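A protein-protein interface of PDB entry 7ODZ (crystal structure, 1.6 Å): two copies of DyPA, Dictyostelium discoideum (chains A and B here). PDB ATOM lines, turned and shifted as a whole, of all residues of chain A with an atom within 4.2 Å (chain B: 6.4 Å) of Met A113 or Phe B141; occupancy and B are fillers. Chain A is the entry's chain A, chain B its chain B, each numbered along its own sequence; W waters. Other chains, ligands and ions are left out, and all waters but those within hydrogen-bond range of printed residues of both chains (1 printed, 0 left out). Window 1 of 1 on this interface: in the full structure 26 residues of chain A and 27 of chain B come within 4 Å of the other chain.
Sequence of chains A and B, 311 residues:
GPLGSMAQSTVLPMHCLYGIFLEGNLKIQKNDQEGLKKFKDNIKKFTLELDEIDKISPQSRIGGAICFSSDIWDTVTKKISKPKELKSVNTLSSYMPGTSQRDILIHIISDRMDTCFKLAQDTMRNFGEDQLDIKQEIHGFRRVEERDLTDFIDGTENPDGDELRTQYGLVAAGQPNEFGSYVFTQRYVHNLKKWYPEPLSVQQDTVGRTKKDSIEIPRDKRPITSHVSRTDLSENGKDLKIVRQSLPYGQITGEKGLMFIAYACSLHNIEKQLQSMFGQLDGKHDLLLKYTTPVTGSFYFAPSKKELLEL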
ATOM      1  N   TYR A  18      13.139   3.674 -13.931  1.00  0.00           N
ATOM      2  CA  TYR A  18      12.820   3.202 -12.587  1.00  0.00           C
ATOM      3  C   TYR A  18      13.890   3.706 -11.642  1.00  0.00           C
ATOM      4  O   TYR A  18      15.046   3.863 -12.030  1.00  0.00           O
ATOM      5  CB  TYR A  18      12.765   1.671 -12.502  1.00  0.00           C
ATOM      6  CG  TYR A  18      11.745   1.142 -13.458  1.00  0.00           C
ATOM      7  CD1 TYR A  18      10.397   1.112 -13.104  1.00  0.00           C
ATOM      8  CD2 TYR A  18      12.102   0.760 -14.746  1.00  0.00           C
ATOM      9  CE1 TYR A  18       9.430   0.687 -14.021  1.00  0.00           C
ATOM     10  CE2 TYR A  18      11.145   0.343 -15.662  1.00  0.00           C
ATOM     11  CZ  TYR A  18       9.810   0.309 -15.290  1.00  0.00           C
ATOM     12  OH  TYR A  18       8.874  -0.085 -16.213  1.00  0.00           O
ATOM     13  N   ARG A 112      14.737  -1.222 -16.174  1.00  0.00           N
ATOM     14  CA  ARG A 112      13.869  -2.363 -15.892  1.00  0.00           C
ATOM     15  C   ARG A 112      13.625  -2.439 -14.394  1.00  0.00           C
ATOM     16  O   ARG A 112      14.578  -2.377 -13.611  1.00  0.00           O
ATOM     17  CB  ARG A 112      14.488  -3.690 -16.353  1.00  0.00           C
ATOM     18  CG  ARG A 112      14.788  -3.776 -17.830  1.00  0.00           C
ATOM     19  CD  ARG A 112      15.439  -5.111 -18.158  1.00  0.00           C
ATOM     20  NE  ARG A 112      14.598  -6.234 -17.734  1.00  0.00           N
ATOM     21  CZ  ARG A 112      13.721  -6.850 -18.522  1.00  0.00           C
ATOM     22  NH1 ARG A 112      13.565  -6.465 -19.796  1.00  0.00           N
ATOM     23  NH2 ARG A 112      12.991  -7.855 -18.037  1.00  0.00           N
ATOM     24  N   MET A 113      12.368  -2.625 -13.983  1.00  0.00           N
ATOM     25  CA  MET A 113      12.137  -2.801 -12.548  1.00  0.00           C
ATOM     26  C   MET A 113      12.785  -4.078 -12.020  1.00  0.00           C
ATOM     27  O   MET A 113      13.240  -4.104 -10.869  1.00  0.00           O
ATOM     28  CB  MET A 113      10.639  -2.797 -12.229  1.00  0.00           C
ATOM     29  CG  MET A 113      10.310  -2.959 -10.751  1.00  0.00           C
ATOM     30  SD  MET A 113      10.944  -1.626  -9.710  1.00  0.00           S
ATOM     31  CE  MET A 113      10.065  -2.022  -8.191  1.00  0.00           C
ATOM     32  N   ASP A 114      12.845  -5.155 -12.820  1.00  0.00           N
ATOM     33  CA  ASP A 114      13.330  -6.398 -12.225  1.00  0.00           C
ATOM     34  C   ASP A 114      14.788  -6.264 -11.775  1.00  0.00           C
ATOM     35  O   ASP A 114      15.141  -6.706 -10.670  1.00  0.00           O
ATOM     36  CB  ASP A 114      13.086  -7.617 -13.145  1.00  0.00           C
ATOM     37  CG  ASP A 114      13.766  -7.551 -14.518  1.00  0.00           C
ATOM     38  OD1 ASP A 114      14.496  -6.604 -14.859  1.00  0.00           O
ATOM     39  OD2 ASP A 114      13.557  -8.530 -15.287  1.00  0.00           O
ATOM     40  N   THR A 115      15.630  -5.577 -12.555  1.00  0.00           N
ATOM     41  CA  THR A 115      17.018  -5.426 -12.116  1.00  0.00           C
ATOM     42  C   THR A 115      17.175  -4.309 -11.087  1.00  0.00           C
ATOM     43  O   THR A 115      18.040  -4.414 -10.203  1.00  0.00           O
ATOM     44  CB  THR A 115      17.934  -5.189 -13.312  1.00  0.00           C
ATOM     45  OG1 THR A 115      17.395  -4.131 -14.102  1.00  0.00           O
ATOM     46  CG2 THR A 115      17.998  -6.438 -14.178  1.00  0.00           C
ATOM     47  N   CYS A 116      16.361  -3.244 -11.169  1.00  0.00           N
ATOM     48  CA  CYS A 116      16.308  -2.260 -10.090  1.00  0.00           C
ATOM     49  C   CYS A 116      16.039  -2.950  -8.761  1.00  0.00           C
ATOM     50  O   CYS A 116      16.777  -2.779  -7.782  1.00  0.00           O
ATOM     51  CB  CYS A 116      15.211  -1.231 -10.395  1.00  0.00           C
ATOM     52  SG  CYS A 116      15.483   0.365  -9.629  1.00  0.00           S
ATOM     53  N   PHE A 117      14.973  -3.745  -8.725  1.00  0.00           N
ATOM     54  CA  PHE A 117      14.562  -4.399  -7.495  1.00  0.00           C
ATOM     55  C   PHE A 117      15.572  -5.445  -7.052  1.00  0.00           C
ATOM     56  O   PHE A 117      15.824  -5.588  -5.847  1.00  0.00           O
ATOM     57  CB  PHE A 117      13.182  -5.024  -7.693  1.00  0.00           C
ATOM     58  CG  PHE A 117      12.582  -5.578  -6.426  1.00  0.00           C
ATOM     59  CD1 PHE A 117      12.795  -6.897  -6.053  1.00  0.00           C
ATOM     60  CD2 PHE A 117      11.773  -4.775  -5.631  1.00  0.00           C
ATOM     61  CE1 PHE A 117      12.244  -7.412  -4.875  1.00  0.00           C
ATOM     62  CE2 PHE A 117      11.188  -5.273  -4.463  1.00  0.00           C
ATOM     63  CZ  PHE A 117      11.428  -6.586  -4.077  1.00  0.00           C
ATOM     64  N   HIS A 139       9.538   3.459  -4.545  1.00  0.00           N
ATOM     65  CA  HIS A 139       9.660   2.870  -5.879  1.00  0.00           C
ATOM     66  C   HIS A 139       9.234   3.932  -6.883  1.00  0.00           C
ATOM     67  O   HIS A 139       8.037   4.134  -7.114  1.00  0.00           O
ATOM     68  CB  HIS A 139       8.795   1.623  -6.002  1.00  0.00           C
ATOM     69  CG  HIS A 139       9.216   0.507  -5.097  1.00  0.00           C
ATOM     70  ND1 HIS A 139       8.549  -0.699  -5.063  1.00  0.00           N
ATOM     71  CD2 HIS A 139      10.214   0.416  -4.183  1.00  0.00           C
ATOM     72  CE1 HIS A 139       9.126  -1.491  -4.174  1.00  0.00           C
ATOM     73  NE2 HIS A 139      10.133  -0.838  -3.621  1.00  0.00           N
ATOM     74  N   CYS B  16       3.910 -11.022 -18.842  1.00  0.00           N
ATOM     75  CA  CYS B  16       3.874  -9.587 -18.555  1.00  0.00           C
ATOM     76  C   CYS B  16       4.908  -9.215 -17.495  1.00  0.00           C
ATOM     77  O   CYS B  16       5.210  -9.981 -16.580  1.00  0.00           O
ATOM     78  CB  CYS B  16       2.481  -9.153 -18.073  1.00  0.00           C
ATOM     79  SG  CYS B  16       1.864 -10.013 -16.577  1.00  0.00           S
ATOM     80  N   LEU B  17       5.450  -8.011 -17.623  1.00  0.00           N
ATOM     81  CA  LEU B  17       6.430  -7.553 -16.652  1.00  0.00           C
ATOM     82  C   LEU B  17       5.815  -6.697 -15.552  1.00  0.00           C
ATOM     83  O   LEU B  17       6.443  -6.532 -14.502  1.00  0.00           O
ATOM     84  CB  LEU B  17       7.551  -6.767 -17.360  1.00  0.00           C
ATOM     85  CG  LEU B  17       8.342  -7.571 -18.408  1.00  0.00           C
ATOM     86  CD1 LEU B  17       9.402  -6.713 -19.082  1.00  0.00           C
ATOM     87  CD2 LEU B  17       8.997  -8.770 -17.718  1.00  0.00           C
ATOM     88  N   TYR B  18       4.608  -6.155 -15.775  1.00  0.00           N
ATOM     89  CA  TYR B  18       3.922  -5.290 -14.823  1.00  0.00           C
ATOM     90  C   TYR B  18       2.444  -5.624 -14.826  1.00  0.00           C
ATOM     91  O   TYR B  18       1.884  -6.021 -15.846  1.00  0.00           O
ATOM     92  CB  TYR B  18       4.108  -3.795 -15.156  1.00  0.00           C
ATOM     93  CG  TYR B  18       5.566  -3.454 -15.218  1.00  0.00           C
ATOM     94  CD1 TYR B  18       6.271  -3.098 -14.062  1.00  0.00           C
ATOM     95  CD2 TYR B  18       6.277  -3.542 -16.412  1.00  0.00           C
ATOM     96  CE1 TYR B  18       7.622  -2.843 -14.102  1.00  0.00           C
ATOM     97  CE2 TYR B  18       7.620  -3.283 -16.456  1.00  0.00           C
ATOM     98  CZ  TYR B  18       8.303  -2.947 -15.296  1.00  0.00           C
ATOM     99  OH  TYR B  18       9.634  -2.707 -15.369  1.00  0.00           O
ATOM    100  N   GLY B  19       1.811  -5.432 -13.674  1.00  0.00           N
ATOM    101  CA  GLY B  19       0.371  -5.586 -13.623  1.00  0.00           C
ATOM    102  C   GLY B  19      -0.175  -4.648 -12.578  1.00  0.00           C
ATOM    103  O   GLY B  19       0.421  -4.511 -11.510  1.00  0.00           O
ATOM    104  N   HIS B 139       0.419  -2.598  -7.307  1.00  0.00           N
ATOM    105  CA  HIS B 139       1.344  -2.491  -8.434  1.00  0.00           C
ATOM    106  C   HIS B 139       2.210  -3.740  -8.421  1.00  0.00           C
ATOM    107  O   HIS B 139       3.134  -3.848  -7.611  1.00  0.00           O
ATOM    108  CB  HIS B 139       2.214  -1.241  -8.340  1.00  0.00           C
ATOM    109  CG  HIS B 139       1.433   0.036  -8.355  1.00  0.00           C
ATOM    110  ND1 HIS B 139       2.025   1.272  -8.172  1.00  0.00           N
ATOM    111  CD2 HIS B 139       0.108   0.271  -8.527  1.00  0.00           C
ATOM    112  CE1 HIS B 139       1.095   2.212  -8.223  1.00  0.00           C
ATOM    113  NE2 HIS B 139      -0.076   1.633  -8.449  1.00  0.00           N
ATOM    114  N   GLY B 140       1.904  -4.684  -9.304  1.00  0.00           N
ATOM    115  CA  GLY B 140       2.694  -5.901  -9.389  1.00  0.00           C
ATOM    116  C   GLY B 140       3.829  -5.745 -10.384  1.00  0.00           C
ATOM    117  O   GLY B 140       3.732  -4.985 -11.351  1.00  0.00           O
ATOM    118  N   PHE B 141       4.926  -6.461 -10.136  1.00  0.00           N
ATOM    119  CA  PHE B 141       6.061  -6.413 -11.050  1.00  0.00           C
ATOM    120  C   PHE B 141       6.739  -7.774 -11.081  1.00  0.00           C
ATOM    121  O   PHE B 141       6.872  -8.443 -10.048  1.00  0.00           O
ATOM    122  CB  PHE B 141       7.086  -5.326 -10.659  1.00  0.00           C
ATOM    123  CG  PHE B 141       7.549  -5.413  -9.229  1.00  0.00           C
ATOM    124  CD1 PHE B 141       6.861  -4.756  -8.228  1.00  0.00           C
ATOM    125  CD2 PHE B 141       8.673  -6.148  -8.892  1.00  0.00           C
ATOM    126  CE1 PHE B 141       7.274  -4.818  -6.906  1.00  0.00           C
ATOM    127  CE2 PHE B 141       9.085  -6.241  -7.567  1.00  0.00           C
ATOM    128  CZ  PHE B 141       8.384  -5.577  -6.568  1.00  0.00           C
ATOM    129  N   ARG B 142       7.172  -8.164 -12.273  1.00  0.00           N
ATOM    130  CA  ARG B 142       7.935  -9.391 -12.432  1.00  0.00           C
ATOM    131  C   ARG B 142       9.349  -9.196 -11.912  1.00  0.00           C
ATOM    132  O   ARG B 142       9.957  -8.136 -12.095  1.00  0.00           O
ATOM    133  CB  ARG B 142       7.979  -9.794 -13.908  1.00  0.00           C
ATOM    134  CG  ARG B 142       8.436 -11.239 -14.128  1.00  0.00           C
ATOM    135  CD  ARG B 142       7.307 -12.224 -13.834  1.00  0.00           C
ATOM    136  NE  ARG B 142       6.226 -12.077 -14.813  1.00  0.00           N
ATOM    137  CZ  ARG B 142       5.174 -12.882 -14.886  1.00  0.00           C
ATOM    138  NH1 ARG B 142       5.062 -13.909 -14.059  1.00  0.00           N
ATOM    139  NH2 ARG B 142       4.227 -12.666 -15.806  1.00  0.00           N
ATOM    140  N   ARG B 143       9.878 -10.233 -11.262  1.00  0.00           N
ATOM    141  CA  ARG B 143      11.247 -10.213 -10.781  1.00  0.00           C
ATOM    142  C   ARG B 143      12.146 -11.009 -11.717  1.00  0.00           C
ATOM    143  O   ARG B 143      11.688 -11.714 -12.626  1.00  0.00           O
ATOM    144  CB  ARG B 143      11.321 -10.771  -9.354  1.00  0.00           C
ATOM    145  CG  ARG B 143      10.799  -9.755  -8.342  1.00  0.00           C
ATOM    146  CD  ARG B 143      10.688 -10.380  -6.957  1.00  0.00           C
ATOM    147  NE  ARG B 143      11.971 -10.637  -6.299  1.00  0.00           N
ATOM    148  CZ  ARG B 143      12.392 -11.839  -5.908  1.00  0.00           C
ATOM    149  NH1 ARG B 143      11.672 -12.926  -6.173  1.00  0.00           N
ATOM    150  NH2 ARG B 143      13.537 -11.966  -5.253  1.00  0.00           N
ATOM    151  N   ARG B 147      10.810 -15.175 -10.562  1.00  0.00           N
ATOM    152  CA  ARG B 147      10.693 -15.777  -9.243  1.00  0.00           C
ATOM    153  C   ARG B 147       9.727 -15.008  -8.351  1.00  0.00           C
ATOM    154  O   ARG B 147       9.735 -13.775  -8.307  1.00  0.00           O
ATOM    155  CB  ARG B 147      12.070 -15.873  -8.583  1.00  0.00           C
ATOM    156  CG  ARG B 147      12.984 -16.877  -9.292  1.00  0.00           C
ATOM    157  CD  ARG B 147      14.386 -16.917  -8.689  1.00  0.00           C
ATOM    158  NE  ARG B 147      15.239 -17.739  -9.542  1.00  0.00           N
ATOM    159  CZ  ARG B 147      15.355 -19.061  -9.448  1.00  0.00           C
ATOM    160  NH1 ARG B 147      14.713 -19.740  -8.502  1.00  0.00           N
ATOM    161  NH2 ARG B 147      16.145 -19.708 -10.292  1.00  0.00           N
ATOM    162  N   LEU B 149       8.644 -14.021  -4.455  1.00  0.00           N
ATOM    163  CA  LEU B 149       9.545 -13.594  -3.383  1.00  0.00           C
ATOM    164  C   LEU B 149      10.002 -14.734  -2.456  1.00  0.00           C
ATOM    165  O   LEU B 149      10.932 -14.521  -1.674  1.00  0.00           O
ATOM    166  CB  LEU B 149       8.879 -12.468  -2.581  1.00  0.00           C
ATOM    167  CG  LEU B 149       8.922 -11.122  -3.320  1.00  0.00           C
ATOM    168  CD1 LEU B 149       7.885 -10.161  -2.751  1.00  0.00           C
ATOM    169  CD2 LEU B 149      10.316 -10.527  -3.186  1.00  0.00           C
ATOM    170  N   LEU B 247       1.672 -11.811  -9.802  1.00  0.00           N
ATOM    171  CA  LEU B 247       2.917 -11.050  -9.793  1.00  0.00           C
ATOM    172  C   LEU B 247       3.310 -10.710  -8.364  1.00  0.00           C
ATOM    173  O   LEU B 247       2.444 -10.419  -7.530  1.00  0.00           O
ATOM    174  CB  LEU B 247       2.791  -9.727 -10.564  1.00  0.00           C
ATOM    175  CG  LEU B 247       2.700  -9.857 -12.090  1.00  0.00           C
ATOM    176  CD1 LEU B 247       2.449  -8.478 -12.684  1.00  0.00           C
ATOM    177  CD2 LEU B 247       3.980 -10.446 -12.672  1.00  0.00           C
ATOM    178  N   PRO B 248       4.611 -10.681  -8.088  1.00  0.00           N
ATOM    179  CA  PRO B 248       5.105 -10.071  -6.841  1.00  0.00           C
ATOM    180  C   PRO B 248       4.667  -8.623  -6.666  1.00  0.00           C
ATOM    181  O   PRO B 248       4.430  -7.889  -7.629  1.00  0.00           O
ATOM    182  CB  PRO B 248       6.627 -10.146  -6.999  1.00  0.00           C
ATOM    183  CG  PRO B 248       6.863 -11.301  -7.963  1.00  0.00           C
ATOM    184  CD  PRO B 248       5.697 -11.230  -8.916  1.00  0.00           C
ATOM    185  N   TYR B 249       4.604  -8.196  -5.410  1.00  0.00           N
ATOM    186  CA  TYR B 249       4.377  -6.781  -5.113  1.00  0.00           C
ATOM    187  C   TYR B 249       5.033  -6.464  -3.775  1.00  0.00           C
ATOM    188  O   TYR B 249       5.342  -7.362  -2.982  1.00  0.00           O
ATOM    189  CB  TYR B 249       2.864  -6.428  -5.049  1.00  0.00           C
ATOM    190  CG  TYR B 249       2.270  -6.942  -3.754  1.00  0.00           C
ATOM    191  CD1 TYR B 249       1.878  -8.277  -3.639  1.00  0.00           C
ATOM    192  CD2 TYR B 249       2.181  -6.131  -2.628  1.00  0.00           C
ATOM    193  CE1 TYR B 249       1.408  -8.777  -2.434  1.00  0.00           C
ATOM    194  CE2 TYR B 249       1.711  -6.620  -1.428  1.00  0.00           C
ATOM    195  CZ  TYR B 249       1.331  -7.946  -1.336  1.00  0.00           C
ATOM    196  OH  TYR B 249       0.874  -8.419  -0.123  1.00  0.00           O
ATOM    197  N   GLY B 250       5.230  -5.177  -3.522  1.00  0.00           N
ATOM    198  CA  GLY B 250       5.470  -4.717  -2.165  1.00  0.00           C
ATOM    199  C   GLY B 250       6.859  -4.140  -1.937  1.00  0.00           C
ATOM    200  O   GLY B 250       7.658  -3.940  -2.851  1.00  0.00           O
ATOM    201  N   GLN B 251       7.139  -3.886  -0.666  1.00  0.00           N
ATOM    202  CA  GLN B 251       8.364  -3.221  -0.239  1.00  0.00           C
ATOM    203  C   GLN B 251       9.363  -4.227   0.305  1.00  0.00           C
ATOM    204  O   GLN B 251       9.008  -5.059   1.142  1.00  0.00           O
ATOM    205  CB  GLN B 251       8.068  -2.198   0.855  1.00  0.00           C
ATOM    206  CG  GLN B 251       6.960  -1.246   0.505  1.00  0.00           C
ATOM    207  CD  GLN B 251       7.492   0.117   0.163  1.00  0.00           C
ATOM    208  OE1 GLN B 251       7.809   0.914   1.051  1.00  0.00           O
ATOM    209  NE2 GLN B 251       7.607   0.397  -1.131  1.00  0.00           N
HETATM  210  O   HOH W   1      11.422 -10.233 -15.060  1.00  0.00           O
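Printed residues of chain B within 4 Å of Met A113: Tyr B18 and Phe B141. Of the printed residues of chain A, Phe B141 touches Met A113 and Phe A117. Of the printed residues of chain A, Gln B251 touches His A139. Of the printed residues of chain B, Asp A114 touches Arg B142 and Arg B143. Printed residues of chain B within 4 Å of Tyr A18: Tyr B18 (2.9 Å). The nearest printed residue of chain B that does not touch Met A113 is Arg B142 (4.9 Å). The nearest printed residue of chain A that does not touch Arg B143 is Met A113 (6.4 Å).
The side-chain hydroxyl of Tyr A18 lies within hydrogen-bond range of the side-chain hydroxyl of Tyr B18 (2.9 Å). N of Met A113 is in hydrogen-bond range of OH of Tyr B18 (3.1 Å).
Water W1 lies within hydrogen-bond range of the side-chain carboxylate of Asp A114 (2.7 Å) and the backbone carbonyl oxygen of Arg B143 (2.9 Å).
The side-chain carboxylate (OD2) of Asp A114 is in salt-bridge range of the guanidinium group (NH2) of Arg A112 (2.9 Å). OG1 of Thr A115 is in hydrogen-bond range of O of Arg A112 (3.4 Å). O of Cys B16 is in hydrogen-bond range of NE of Arg B142 (2.9 Å). N of Arg B142 lies within hydrogen-bond range of O of Leu B17, 2.9 Å away. O of Pro B248 lies within hydrogen-bond range of N of Phe B141. NH1 of Arg B143 lies within hydrogen-bond range of O of Arg B147 (3.0 Å).
Of the 16 printed residues of chain B, 7 touch a printed residue of chain A. Hydrophobic or aromatic side chains of chain B within 4 Å of the printed part of chain A: Leu B17, Tyr B18 and Phe B141.
Arg A112 touches Leu B17. Met A113 touches Phe B141. Asp A114 touches Arg B142. Arg B143 touches Asp A114. CE2 of Phe A117 touches CZ of Phe B141, at 3.5 Å. Phe A117 touches Arg B143 (CE1 to NE, 3.5 Å). CE1 of His A139 touches O of Gly B250 (3.1 Å). His A139 touches Gln B251.
Tyr A18 touches its own counterpart, Tyr B18. Positions printed for both chains: 18 and 139. Of the 10 pairs that touch across the chains among the printed residues, 1 has its exchanged pair printed and touching as well.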
